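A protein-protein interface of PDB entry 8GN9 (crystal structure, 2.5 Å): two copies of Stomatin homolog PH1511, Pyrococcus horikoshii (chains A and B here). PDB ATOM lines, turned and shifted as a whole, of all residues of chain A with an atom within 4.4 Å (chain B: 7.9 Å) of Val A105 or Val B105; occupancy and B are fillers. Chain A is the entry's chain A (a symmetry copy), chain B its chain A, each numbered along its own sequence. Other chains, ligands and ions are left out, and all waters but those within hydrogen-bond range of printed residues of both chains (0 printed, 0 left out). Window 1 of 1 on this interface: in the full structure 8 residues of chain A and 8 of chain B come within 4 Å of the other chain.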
ATOM      1  N   ARG A  25      26.237 -22.279   8.019  1.00  0.00           N
ATOM      2  CA  ARG A  25      25.125 -23.216   8.325  1.00  0.00           C
ATOM      3  C   ARG A  25      23.837 -22.389   8.291  1.00  0.00           C
ATOM      4  O   ARG A  25      23.711 -21.455   9.115  1.00  0.00           O
ATOM      5  CB  ARG A  25      25.312 -23.868   9.698  1.00  0.00           C
ATOM      6  CG  ARG A  25      26.326 -25.000   9.745  1.00  0.00           C
ATOM      7  CD  ARG A  25      26.376 -25.666  11.112  1.00  0.00           C
ATOM      8  NE  ARG A  25      26.279 -27.107  10.912  1.00  0.00           N
ATOM      9  CZ  ARG A  25      25.193 -27.854  11.108  1.00  0.00           C
ATOM     10  NH1 ARG A  25      24.071 -27.321  11.569  1.00  0.00           N
ATOM     11  NH2 ARG A  25      25.245 -29.153  10.857  1.00  0.00           N
ATOM     12  N   VAL A  26      22.948 -22.677   7.342  1.00  0.00           N
ATOM     13  CA  VAL A  26      21.731 -21.858   7.072  1.00  0.00           C
ATOM     14  C   VAL A  26      20.501 -22.752   7.075  1.00  0.00           C
ATOM     15  O   VAL A  26      20.578 -23.879   6.549  1.00  0.00           O
ATOM     16  CB  VAL A  26      21.823 -21.081   5.750  1.00  0.00           C
ATOM     17  CG1 VAL A  26      20.676 -20.099   5.631  1.00  0.00           C
ATOM     18  CG2 VAL A  26      23.152 -20.363   5.630  1.00  0.00           C
ATOM     19  N   LEU A  71      24.414 -11.857   2.945  1.00  0.00           N
ATOM     20  CA  LEU A  71      23.809 -12.454   4.164  1.00  0.00           C
ATOM     21  C   LEU A  71      23.608 -11.376   5.240  1.00  0.00           C
ATOM     22  O   LEU A  71      22.600 -11.443   5.949  1.00  0.00           O
ATOM     23  CB  LEU A  71      24.696 -13.578   4.701  1.00  0.00           C
ATOM     24  CG  LEU A  71      24.599 -14.908   3.960  1.00  0.00           C
ATOM     25  CD1 LEU A  71      25.703 -15.848   4.417  1.00  0.00           C
ATOM     26  CD2 LEU A  71      23.242 -15.554   4.178  1.00  0.00           C
ATOM     27  N   ARG A  75      19.538  -9.459   3.186  1.00  0.00           N
ATOM     28  CA  ARG A  75      18.693 -10.613   3.603  1.00  0.00           C
ATOM     29  C   ARG A  75      17.419 -10.652   2.754  1.00  0.00           C
ATOM     30  O   ARG A  75      17.150 -11.696   2.144  1.00  0.00           O
ATOM     31  CB  ARG A  75      18.272 -10.482   5.069  1.00  0.00           C
ATOM     32  CG  ARG A  75      19.214 -11.144   6.059  1.00  0.00           C
ATOM     33  CD  ARG A  75      19.003 -12.648   6.087  1.00  0.00           C
ATOM     34  NE  ARG A  75      18.972 -13.180   7.445  1.00  0.00           N
ATOM     35  CZ  ARG A  75      20.026 -13.313   8.239  1.00  0.00           C
ATOM     36  NH1 ARG A  75      19.866 -13.817   9.453  1.00  0.00           N
ATOM     37  NH2 ARG A  75      21.227 -12.946   7.823  1.00  0.00           N
ATOM     38  N   ILE A 102      15.026 -16.930   5.390  1.00  0.00           N
ATOM     39  CA  ILE A 102      16.239 -17.462   6.057  1.00  0.00           C
ATOM     40  C   ILE A 102      16.071 -17.107   7.537  1.00  0.00           C
ATOM     41  O   ILE A 102      15.722 -15.948   7.828  1.00  0.00           O
ATOM     42  CB  ILE A 102      17.516 -16.876   5.414  1.00  0.00           C
ATOM     43  CG1 ILE A 102      17.670 -17.319   3.950  1.00  0.00           C
ATOM     44  CG2 ILE A 102      18.746 -17.227   6.228  1.00  0.00           C
ATOM     45  CD1 ILE A 102      18.633 -16.468   3.123  1.00  0.00           C
ATOM     46  N   LYS A 103      16.184 -18.086   8.430  1.00  0.00           N
ATOM     47  CA  LYS A 103      16.142 -17.826   9.886  1.00  0.00           C
ATOM     48  C   LYS A 103      17.576 -17.607  10.376  1.00  0.00           C
ATOM     49  O   LYS A 103      18.089 -16.475  10.285  1.00  0.00           O
ATOM     50  CB  LYS A 103      15.497 -18.991  10.630  1.00  0.00           C
ATOM     51  CG  LYS A 103      14.024 -19.213  10.364  1.00  0.00           C
ATOM     52  CD  LYS A 103      13.570 -20.514  10.989  1.00  0.00           C
ATOM     53  CE  LYS A 103      13.472 -20.468  12.502  1.00  0.00           C
ATOM     54  NZ  LYS A 103      12.853 -21.712  13.023  1.00  0.00           N
ATOM     55  N   ASP A 104      18.210 -18.685  10.821  1.00  0.00           N
ATOM     56  CA  ASP A 104      19.524 -18.668  11.494  1.00  0.00           C
ATOM     57  C   ASP A 104      20.597 -18.751  10.408  1.00  0.00           C
ATOM     58  O   ASP A 104      20.331 -19.346   9.339  1.00  0.00           O
ATOM     59  CB  ASP A 104      19.585 -19.797  12.527  1.00  0.00           C
ATOM     60  CG  ASP A 104      18.383 -19.806  13.460  1.00  0.00           C
ATOM     61  OD1 ASP A 104      17.884 -18.708  13.780  1.00  0.00           O
ATOM     62  OD2 ASP A 104      17.943 -20.906  13.847  1.00  0.00           O
ATOM     63  N   VAL A 105      21.738 -18.117  10.659  1.00  0.00           N
ATOM     64  CA  VAL A 105      22.969 -18.204   9.821  1.00  0.00           C
ATOM     65  C   VAL A 105      24.140 -18.400  10.790  1.00  0.00           C
ATOM     66  O   VAL A 105      24.525 -17.412  11.442  1.00  0.00           O
ATOM     67  CB  VAL A 105      23.160 -16.940   8.957  1.00  0.00           C
ATOM     68  CG1 VAL A 105      24.421 -17.012   8.103  1.00  0.00           C
ATOM     69  CG2 VAL A 105      21.939 -16.654   8.102  1.00  0.00           C
ATOM     70  N   GLU A 106      24.645 -19.626  10.918  1.00  0.00           N
ATOM     71  CA  GLU A 106      25.765 -19.948  11.827  1.00  0.00           C
ATOM     72  C   GLU A 106      27.040 -19.937  10.996  1.00  0.00           C
ATOM     73  O   GLU A 106      26.987 -20.388   9.858  1.00  0.00           O
ATOM     74  CB  GLU A 106      25.580 -21.301  12.515  1.00  0.00           C
ATOM     75  CG  GLU A 106      24.388 -21.352  13.455  1.00  0.00           C
ATOM     76  CD  GLU A 106      24.187 -22.691  14.149  1.00  0.00           C
ATOM     77  OE1 GLU A 106      25.143 -23.515  14.160  1.00  0.00           O
ATOM     78  OE2 GLU A 106      23.067 -22.913  14.663  1.00  0.00           O
ATOM     79  N   LEU A 107      28.116 -19.395  11.559  1.00  0.00           N
ATOM     80  CA  LEU A 107      29.498 -19.447  11.021  1.00  0.00           C
ATOM     81  C   LEU A 107      30.290 -20.424  11.887  1.00  0.00           C
ATOM     82  O   LEU A 107      30.702 -20.067  12.988  1.00  0.00           O
ATOM     83  CB  LEU A 107      30.094 -18.042  11.084  1.00  0.00           C
ATOM     84  CG  LEU A 107      29.241 -16.924  10.487  1.00  0.00           C
ATOM     85  CD1 LEU A 107      29.489 -15.597  11.198  1.00  0.00           C
ATOM     86  CD2 LEU A 107      29.500 -16.781   8.998  1.00  0.00           C
ATOM     87  N   THR B  18      28.687  -6.474  17.172  1.00  0.00           N
ATOM     88  CA  THR B  18      30.144  -6.304  16.975  1.00  0.00           C
ATOM     89  C   THR B  18      30.451  -4.804  16.957  1.00  0.00           C
ATOM     90  O   THR B  18      29.495  -3.993  16.978  1.00  0.00           O
ATOM     91  CB  THR B  18      30.611  -6.990  15.689  1.00  0.00           C
ATOM     92  OG1 THR B  18      30.146  -6.184  14.604  1.00  0.00           O
ATOM     93  CG2 THR B  18      30.130  -8.427  15.585  1.00  0.00           C
ATOM     94  N   VAL B  22      27.422  -5.270  13.764  1.00  0.00           N
ATOM     95  CA  VAL B  22      26.817  -6.543  13.282  1.00  0.00           C
ATOM     96  C   VAL B  22      26.202  -7.267  14.472  1.00  0.00           C
ATOM     97  O   VAL B  22      26.894  -7.638  15.416  1.00  0.00           O
ATOM     98  CB  VAL B  22      27.800  -7.432  12.505  1.00  0.00           C
ATOM     99  CG1 VAL B  22      27.105  -8.696  12.018  1.00  0.00           C
ATOM    100  CG2 VAL B  22      28.429  -6.682  11.341  1.00  0.00           C
ATOM    101  N   PRO B  23      24.869  -7.491  14.442  1.00  0.00           N
ATOM    102  CA  PRO B  23      24.201  -8.327  15.437  1.00  0.00           C
ATOM    103  C   PRO B  23      24.716  -9.773  15.344  1.00  0.00           C
ATOM    104  O   PRO B  23      24.765 -10.327  14.255  1.00  0.00           O
ATOM    105  CB  PRO B  23      22.711  -8.227  15.067  1.00  0.00           C
ATOM    106  CG  PRO B  23      22.623  -6.997  14.185  1.00  0.00           C
ATOM    107  CD  PRO B  23      23.932  -6.970  13.435  1.00  0.00           C
ATOM    108  N   VAL B  24      25.094 -10.341  16.486  1.00  0.00           N
ATOM    109  CA  VAL B  24      25.641 -11.725  16.604  1.00  0.00           C
ATOM    110  C   VAL B  24      24.981 -12.400  17.803  1.00  0.00           C
ATOM    111  O   VAL B  24      24.810 -11.735  18.812  1.00  0.00           O
ATOM    112  CB  VAL B  24      27.173 -11.701  16.745  1.00  0.00           C
ATOM    113  CG1 VAL B  24      27.846 -11.282  15.453  1.00  0.00           C
ATOM    114  CG2 VAL B  24      27.624 -10.797  17.884  1.00  0.00           C
ATOM    115  N   ARG B  25      24.590 -13.663  17.651  1.00  0.00           N
ATOM    116  CA  ARG B  25      24.195 -14.583  18.749  1.00  0.00           C
ATOM    117  C   ARG B  25      25.344 -15.582  18.912  1.00  0.00           C
ATOM    118  O   ARG B  25      25.622 -16.328  17.947  1.00  0.00           O
ATOM    119  CB  ARG B  25      22.890 -15.311  18.419  1.00  0.00           C
ATOM    120  CG  ARG B  25      21.624 -14.489  18.606  1.00  0.00           C
ATOM    121  CD  ARG B  25      20.367 -15.312  18.365  1.00  0.00           C
ATOM    122  NE  ARG B  25      19.468 -15.099  19.492  1.00  0.00           N
ATOM    123  CZ  ARG B  25      19.262 -15.945  20.501  1.00  0.00           C
ATOM    124  NH1 ARG B  25      19.857 -17.128  20.532  1.00  0.00           N
ATOM    125  NH2 ARG B  25      18.433 -15.604  21.476  1.00  0.00           N
ATOM    126  N   VAL B  26      26.020 -15.556  20.060  1.00  0.00           N
ATOM    127  CA  VAL B  26      27.264 -16.343  20.305  1.00  0.00           C
ATOM    128  C   VAL B  26      27.117 -17.148  21.587  1.00  0.00           C
ATOM    129  O   VAL B  26      26.554 -16.619  22.565  1.00  0.00           O
ATOM    130  CB  VAL B  26      28.519 -15.458  20.372  1.00  0.00           C
ATOM    131  CG1 VAL B  26      29.769 -16.313  20.394  1.00  0.00           C
ATOM    132  CG2 VAL B  26      28.562 -14.484  19.212  1.00  0.00           C
ATOM    133  N   ASN B  27      27.612 -18.381  21.546  1.00  0.00           N
ATOM    134  CA  ASN B  27      27.755 -19.263  22.731  1.00  0.00           C
ATOM    135  C   ASN B  27      29.148 -19.895  22.676  1.00  0.00           C
ATOM    136  O   ASN B  27      29.864 -19.717  21.657  1.00  0.00           O
ATOM    137  CB  ASN B  27      26.628 -20.301  22.816  1.00  0.00           C
ATOM    138  CG  ASN B  27      26.571 -21.246  21.631  1.00  0.00           C
ATOM    139  OD1 ASN B  27      27.238 -21.031  20.619  1.00  0.00           O
ATOM    140  ND2 ASN B  27      25.766 -22.291  21.745  1.00  0.00           N
ATOM    141  N   ILE B  63      33.233  -9.939  22.417  1.00  0.00           N
ATOM    142  CA  ILE B  63      32.602  -9.985  21.070  1.00  0.00           C
ATOM    143  C   ILE B  63      32.080  -8.596  20.686  1.00  0.00           C
ATOM    144  O   ILE B  63      32.206  -8.229  19.489  1.00  0.00           O
ATOM    145  CB  ILE B  63      31.532 -11.091  21.068  1.00  0.00           C
ATOM    146  CG1 ILE B  63      32.244 -12.446  21.014  1.00  0.00           C
ATOM    147  CG2 ILE B  63      30.519 -10.904  19.943  1.00  0.00           C
ATOM    148  CD1 ILE B  63      31.323 -13.616  20.980  1.00  0.00           C
ATOM    149  N   LEU B  68      33.503  -8.272  13.060  1.00  0.00           N
ATOM    150  CA  LEU B  68      33.003  -9.529  12.453  1.00  0.00           C
ATOM    151  C   LEU B  68      34.177 -10.290  11.826  1.00  0.00           C
ATOM    152  O   LEU B  68      34.221 -11.519  11.966  1.00  0.00           O
ATOM    153  CB  LEU B  68      31.933  -9.206  11.410  1.00  0.00           C
ATOM    154  CG  LEU B  68      31.346 -10.418  10.685  1.00  0.00           C
ATOM    155  CD1 LEU B  68      30.765 -11.419  11.671  1.00  0.00           C
ATOM    156  CD2 LEU B  68      30.290  -9.985   9.683  1.00  0.00           C
ATOM    157  N   LEU B  71      35.710 -12.618  14.057  1.00  0.00           N
ATOM    158  CA  LEU B  71      34.854 -13.824  14.201  1.00  0.00           C
ATOM    159  C   LEU B  71      35.129 -14.810  13.056  1.00  0.00           C
ATOM    160  O   LEU B  71      35.104 -16.018  13.310  1.00  0.00           O
ATOM    161  CB  LEU B  71      33.377 -13.427  14.214  1.00  0.00           C
ATOM    162  CG  LEU B  71      32.857 -12.858  15.530  1.00  0.00           C
ATOM    163  CD1 LEU B  71      31.469 -12.269  15.338  1.00  0.00           C
ATOM    164  CD2 LEU B  71      32.823 -13.928  16.608  1.00  0.00           C
ATOM    165  N   LEU B  72      35.361 -14.324  11.839  1.00  0.00           N
ATOM    166  CA  LEU B  72      35.637 -15.179  10.653  1.00  0.00           C
ATOM    167  C   LEU B  72      37.071 -15.711  10.750  1.00  0.00           C
ATOM    168  O   LEU B  72      37.237 -16.927  10.940  1.00  0.00           O
ATOM    169  CB  LEU B  72      35.427 -14.361   9.372  1.00  0.00           C
ATOM    170  CG  LEU B  72      34.068 -13.679   9.246  1.00  0.00           C
ATOM    171  CD1 LEU B  72      34.002 -12.836   7.984  1.00  0.00           C
ATOM    172  CD2 LEU B  72      32.949 -14.704   9.269  1.00  0.00           C
ATOM    173  N   ARG B  75      39.322 -16.575  14.995  1.00  0.00           N
ATOM    174  CA  ARG B  75      38.600 -17.354  16.039  1.00  0.00           C
ATOM    175  C   ARG B  75      39.561 -17.702  17.180  1.00  0.00           C
ATOM    176  O   ARG B  75      39.246 -17.376  18.333  1.00  0.00           O
ATOM    177  CB  ARG B  75      38.061 -18.668  15.467  1.00  0.00           C
ATOM    178  CG  ARG B  75      36.649 -18.587  14.916  1.00  0.00           C
ATOM    179  CD  ARG B  75      35.625 -18.605  16.038  1.00  0.00           C
ATOM    180  NE  ARG B  75      34.504 -19.493  15.755  1.00  0.00           N
ATOM    181  CZ  ARG B  75      33.538 -19.252  14.878  1.00  0.00           C
ATOM    182  NH1 ARG B  75      32.570 -20.140  14.716  1.00  0.00           N
ATOM    183  NH2 ARG B  75      33.542 -18.133  14.171  1.00  0.00           N
ATOM    184  N   LEU B  78      40.437 -14.974  19.515  1.00  0.00           N
ATOM    185  CA  LEU B  78      39.276 -14.579  20.360  1.00  0.00           C
ATOM    186  C   LEU B  78      39.144 -15.583  21.506  1.00  0.00           C
ATOM    187  O   LEU B  78      38.887 -15.157  22.632  1.00  0.00           O
ATOM    188  CB  LEU B  78      37.990 -14.505  19.523  1.00  0.00           C
ATOM    189  CG  LEU B  78      37.867 -13.332  18.538  1.00  0.00           C
ATOM    190  CD1 LEU B  78      36.474 -13.283  17.924  1.00  0.00           C
ATOM    191  CD2 LEU B  78      38.158 -11.997  19.197  1.00  0.00           C
ATOM    192  N   ILE B 102      34.524 -20.586  21.470  1.00  0.00           N
ATOM    193  CA  ILE B 102      33.272 -20.101  20.839  1.00  0.00           C
ATOM    194  C   ILE B 102      32.785 -21.264  19.969  1.00  0.00           C
ATOM    195  O   ILE B 102      33.612 -21.834  19.233  1.00  0.00           O
ATOM    196  CB  ILE B 102      33.529 -18.796  20.052  1.00  0.00           C
ATOM    197  CG1 ILE B 102      33.949 -17.646  20.981  1.00  0.00           C
ATOM    198  CG2 ILE B 102      32.321 -18.417  19.217  1.00  0.00           C
ATOM    199  CD1 ILE B 102      34.627 -16.472  20.277  1.00  0.00           C
ATOM    200  N   LYS B 103      31.536 -21.687  20.135  1.00  0.00           N
ATOM    201  CA  LYS B 103      30.942 -22.731  19.272  1.00  0.00           C
ATOM    202  C   LYS B 103      30.244 -22.043  18.097  1.00  0.00           C
ATOM    203  O   LYS B 103      30.907 -21.724  17.091  1.00  0.00           O
ATOM    204  CB  LYS B 103      29.949 -23.586  20.055  1.00  0.00           C
ATOM    205  CG  LYS B 103      30.538 -24.455  21.145  1.00  0.00           C
ATOM    206  CD  LYS B 103      29.434 -25.075  21.972  1.00  0.00           C
ATOM    207  CE  LYS B 103      28.675 -26.178  21.258  1.00  0.00           C
ATOM    208  NZ  LYS B 103      27.737 -26.853  22.189  1.00  0.00           N
ATOM    209  N   ASP B 104      28.955 -21.773  18.262  1.00  0.00           N
ATOM    210  CA  ASP B 104      28.058 -21.275  17.200  1.00  0.00           C
ATOM    211  C   ASP B 104      28.155 -19.749  17.196  1.00  0.00           C
ATOM    212  O   ASP B 104      28.419 -19.156  18.266  1.00  0.00           O
ATOM    213  CB  ASP B 104      26.644 -21.815  17.429  1.00  0.00           C
ATOM    214  CG  ASP B 104      26.616 -23.322  17.641  1.00  0.00           C
ATOM    215  OD1 ASP B 104      27.444 -24.015  17.015  1.00  0.00           O
ATOM    216  OD2 ASP B 104      25.783 -23.792  18.441  1.00  0.00           O
ATOM    217  N   VAL B 105      28.010 -19.154  16.016  1.00  0.00           N
ATOM    218  CA  VAL B 105      27.903 -17.681  15.806  1.00  0.00           C
ATOM    219  C   VAL B 105      26.747 -17.466  14.823  1.00  0.00           C
ATOM    220  O   VAL B 105      26.950 -17.730  13.623  1.00  0.00           O
ATOM    221  CB  VAL B 105      29.220 -17.086  15.265  1.00  0.00           C
ATOM    222  CG1 VAL B 105      29.120 -15.582  15.036  1.00  0.00           C
ATOM    223  CG2 VAL B 105      30.399 -17.424  16.158  1.00  0.00           C
ATOM    224  N   GLU B 106      25.578 -17.060  15.315  1.00  0.00           N
ATOM    225  CA  GLU B 106      24.384 -16.828  14.474  1.00  0.00           C
ATOM    226  C   GLU B 106      24.327 -15.338  14.169  1.00  0.00           C
ATOM    227  O   GLU B 106      24.647 -14.559  15.060  1.00  0.00           O
ATOM    228  CB  GLU B 106      23.098 -17.291  15.157  1.00  0.00           C
ATOM    229  CG  GLU B 106      23.032 -18.790  15.389  1.00  0.00           C
ATOM    230  CD  GLU B 106      21.759 -19.270  16.070  1.00  0.00           C
ATOM    231  OE1 GLU B 106      20.761 -18.497  16.098  1.00  0.00           O
ATOM    232  OE2 GLU B 106      21.773 -20.411  16.586  1.00  0.00           O
ATOM    233  N   LEU B 107      23.970 -14.993  12.935  1.00  0.00           N
ATOM    234  CA  LEU B 107      23.662 -13.617  12.474  1.00  0.00           C
ATOM    235  C   LEU B 107      22.150 -13.528  12.278  1.00  0.00           C
ATOM    236  O   LEU B 107      21.635 -14.011  11.273  1.00  0.00           O
ATOM    237  CB  LEU B 107      24.406 -13.370  11.162  1.00  0.00           C
ATOM    238  CG  LEU B 107      25.897 -13.701  11.164  1.00  0.00           C
ATOM    239  CD1 LEU B 107      26.370 -14.139   9.781  1.00  0.00           C
ATOM    240  CD2 LEU B 107      26.714 -12.517  11.650  1.00  0.00           C
ATOM    241  N   PRO B 108      21.383 -12.989  13.256  1.00  0.00           N
ATOM    242  CA  PRO B 108      19.942 -12.761  13.083  1.00  0.00           C
ATOM    243  C   PRO B 108      19.572 -11.675  12.055  1.00  0.00           C
ATOM    244  O   PRO B 108      20.296 -10.682  11.917  1.00  0.00           O
ATOM    245  CB  PRO B 108      19.500 -12.308  14.483  1.00  0.00           C
ATOM    246  CG  PRO B 108      20.568 -12.851  15.395  1.00  0.00           C
ATOM    247  CD  PRO B 108      21.844 -12.650  14.608  1.00  0.00           C
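O of Val A105 lies close to O of Val B105. OE2 of Glu A106 sits close to OE2 of Glu B106 (3.4 Å). The backbone NH of Leu A107 sits at hydrogen-bond distance from the backbone carbonyl oxygen of Val B105 (2.9 Å). The guanidinium group (NH1) of Arg A75 sits at hydrogen-bond distance from the backbone carbonyl oxygen (O) of Leu B107, at 2.5 Å. The guanidinium group (NH1) of Arg B75 lies within hydrogen-bond range of the backbone carbonyl oxygen (O) of Leu A107. The backbone carbonyl oxygen (O) of Val A105 is in hydrogen-bond range of the backbone NH (N) of Leu B107 (2.9 Å).
The backbone carbonyl oxygen (O) of Arg A25 lies within hydrogen-bond range of the backbone NH (N) of Glu A106 (2.7 Å). The guanidinium group of Arg A75 is in hydrogen-bond range of the backbone carbonyl oxygen of Lys A103, 3.3 Å away. The backbone carbonyl oxygen (O) of Arg B25 is in hydrogen-bond range of the backbone NH (N) of Glu B106, 2.7 Å away. The side-chain amide oxygen (OD1) of Asn B27 lies within hydrogen-bond range of the backbone NH (N) of Asp B104 (3.0 Å). The backbone carbonyl oxygen (O) of Leu B71 is in hydrogen-bond range of the guanidinium group (NH2) of Arg B75, 2.8 Å away. The guanidinium group (NH1) of Arg B75 is in hydrogen-bond range of the backbone carbonyl oxygen (O) of Lys B103, 3.3 Å away.
Arg A75 touches Pro B108. Asp A104 touches Glu B106. Val A105 touches Glu B106. Glu A106 touches Asp B104 (OE1 to OD1, 3.7 Å). CA of Glu A106 touches O of Val B105, 3.1 Å away. Leu A107 touches Leu B107 (CD1 to CD1, 3.7 Å).
Val A105 touches just these residues of chain B: Val B105, Glu B106 and Leu B107. Asn B27 touches none of the printed residues of chain A. Leu B68 touches none of the printed residues of chain A. Printed residues of chain A within 4 Å of Asp B104: Glu A106. Val B105 touches just these residues of chain A: Val A105 (3.3 Å), Glu A106 (3.1 Å) and Leu A107 (2.9 Å). Printed residues of chain A within 4 Å of Glu B106: Asp A104, Val A105 and Glu A106. Of the printed residues of chain A, Pro B108 touches Arg A75 (3.4 Å). The nearest residue of chain B that does not touch Val A105 is Pro B108 (5.7 Å). The nearest printed residue of chain A that does not touch Val B105 is Arg A25 (6.7 Å). The nearest printed residue of chain B that does not touch Asp A104 is Leu B107 (4.9 Å).
Along chain B the printed residues that touch a printed residue of chain A span positions 75 to 108. Among the printed residues, no Asp or Glu carboxylate lies within 4 Å of a Lys or Arg side-chain nitrogen of the other chain.
Arg A75 touches Leu B107, and with the chains exchanged Leu A107 touches Arg B75. Asp A104 touches Glu B106, and with the chains exchanged Glu A106 touches Asp B104. Val A105 touches Leu B107, and with the chains exchanged Leu A107 touches Val B105. Leu B107 touches its own counterpart, Leu A107.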
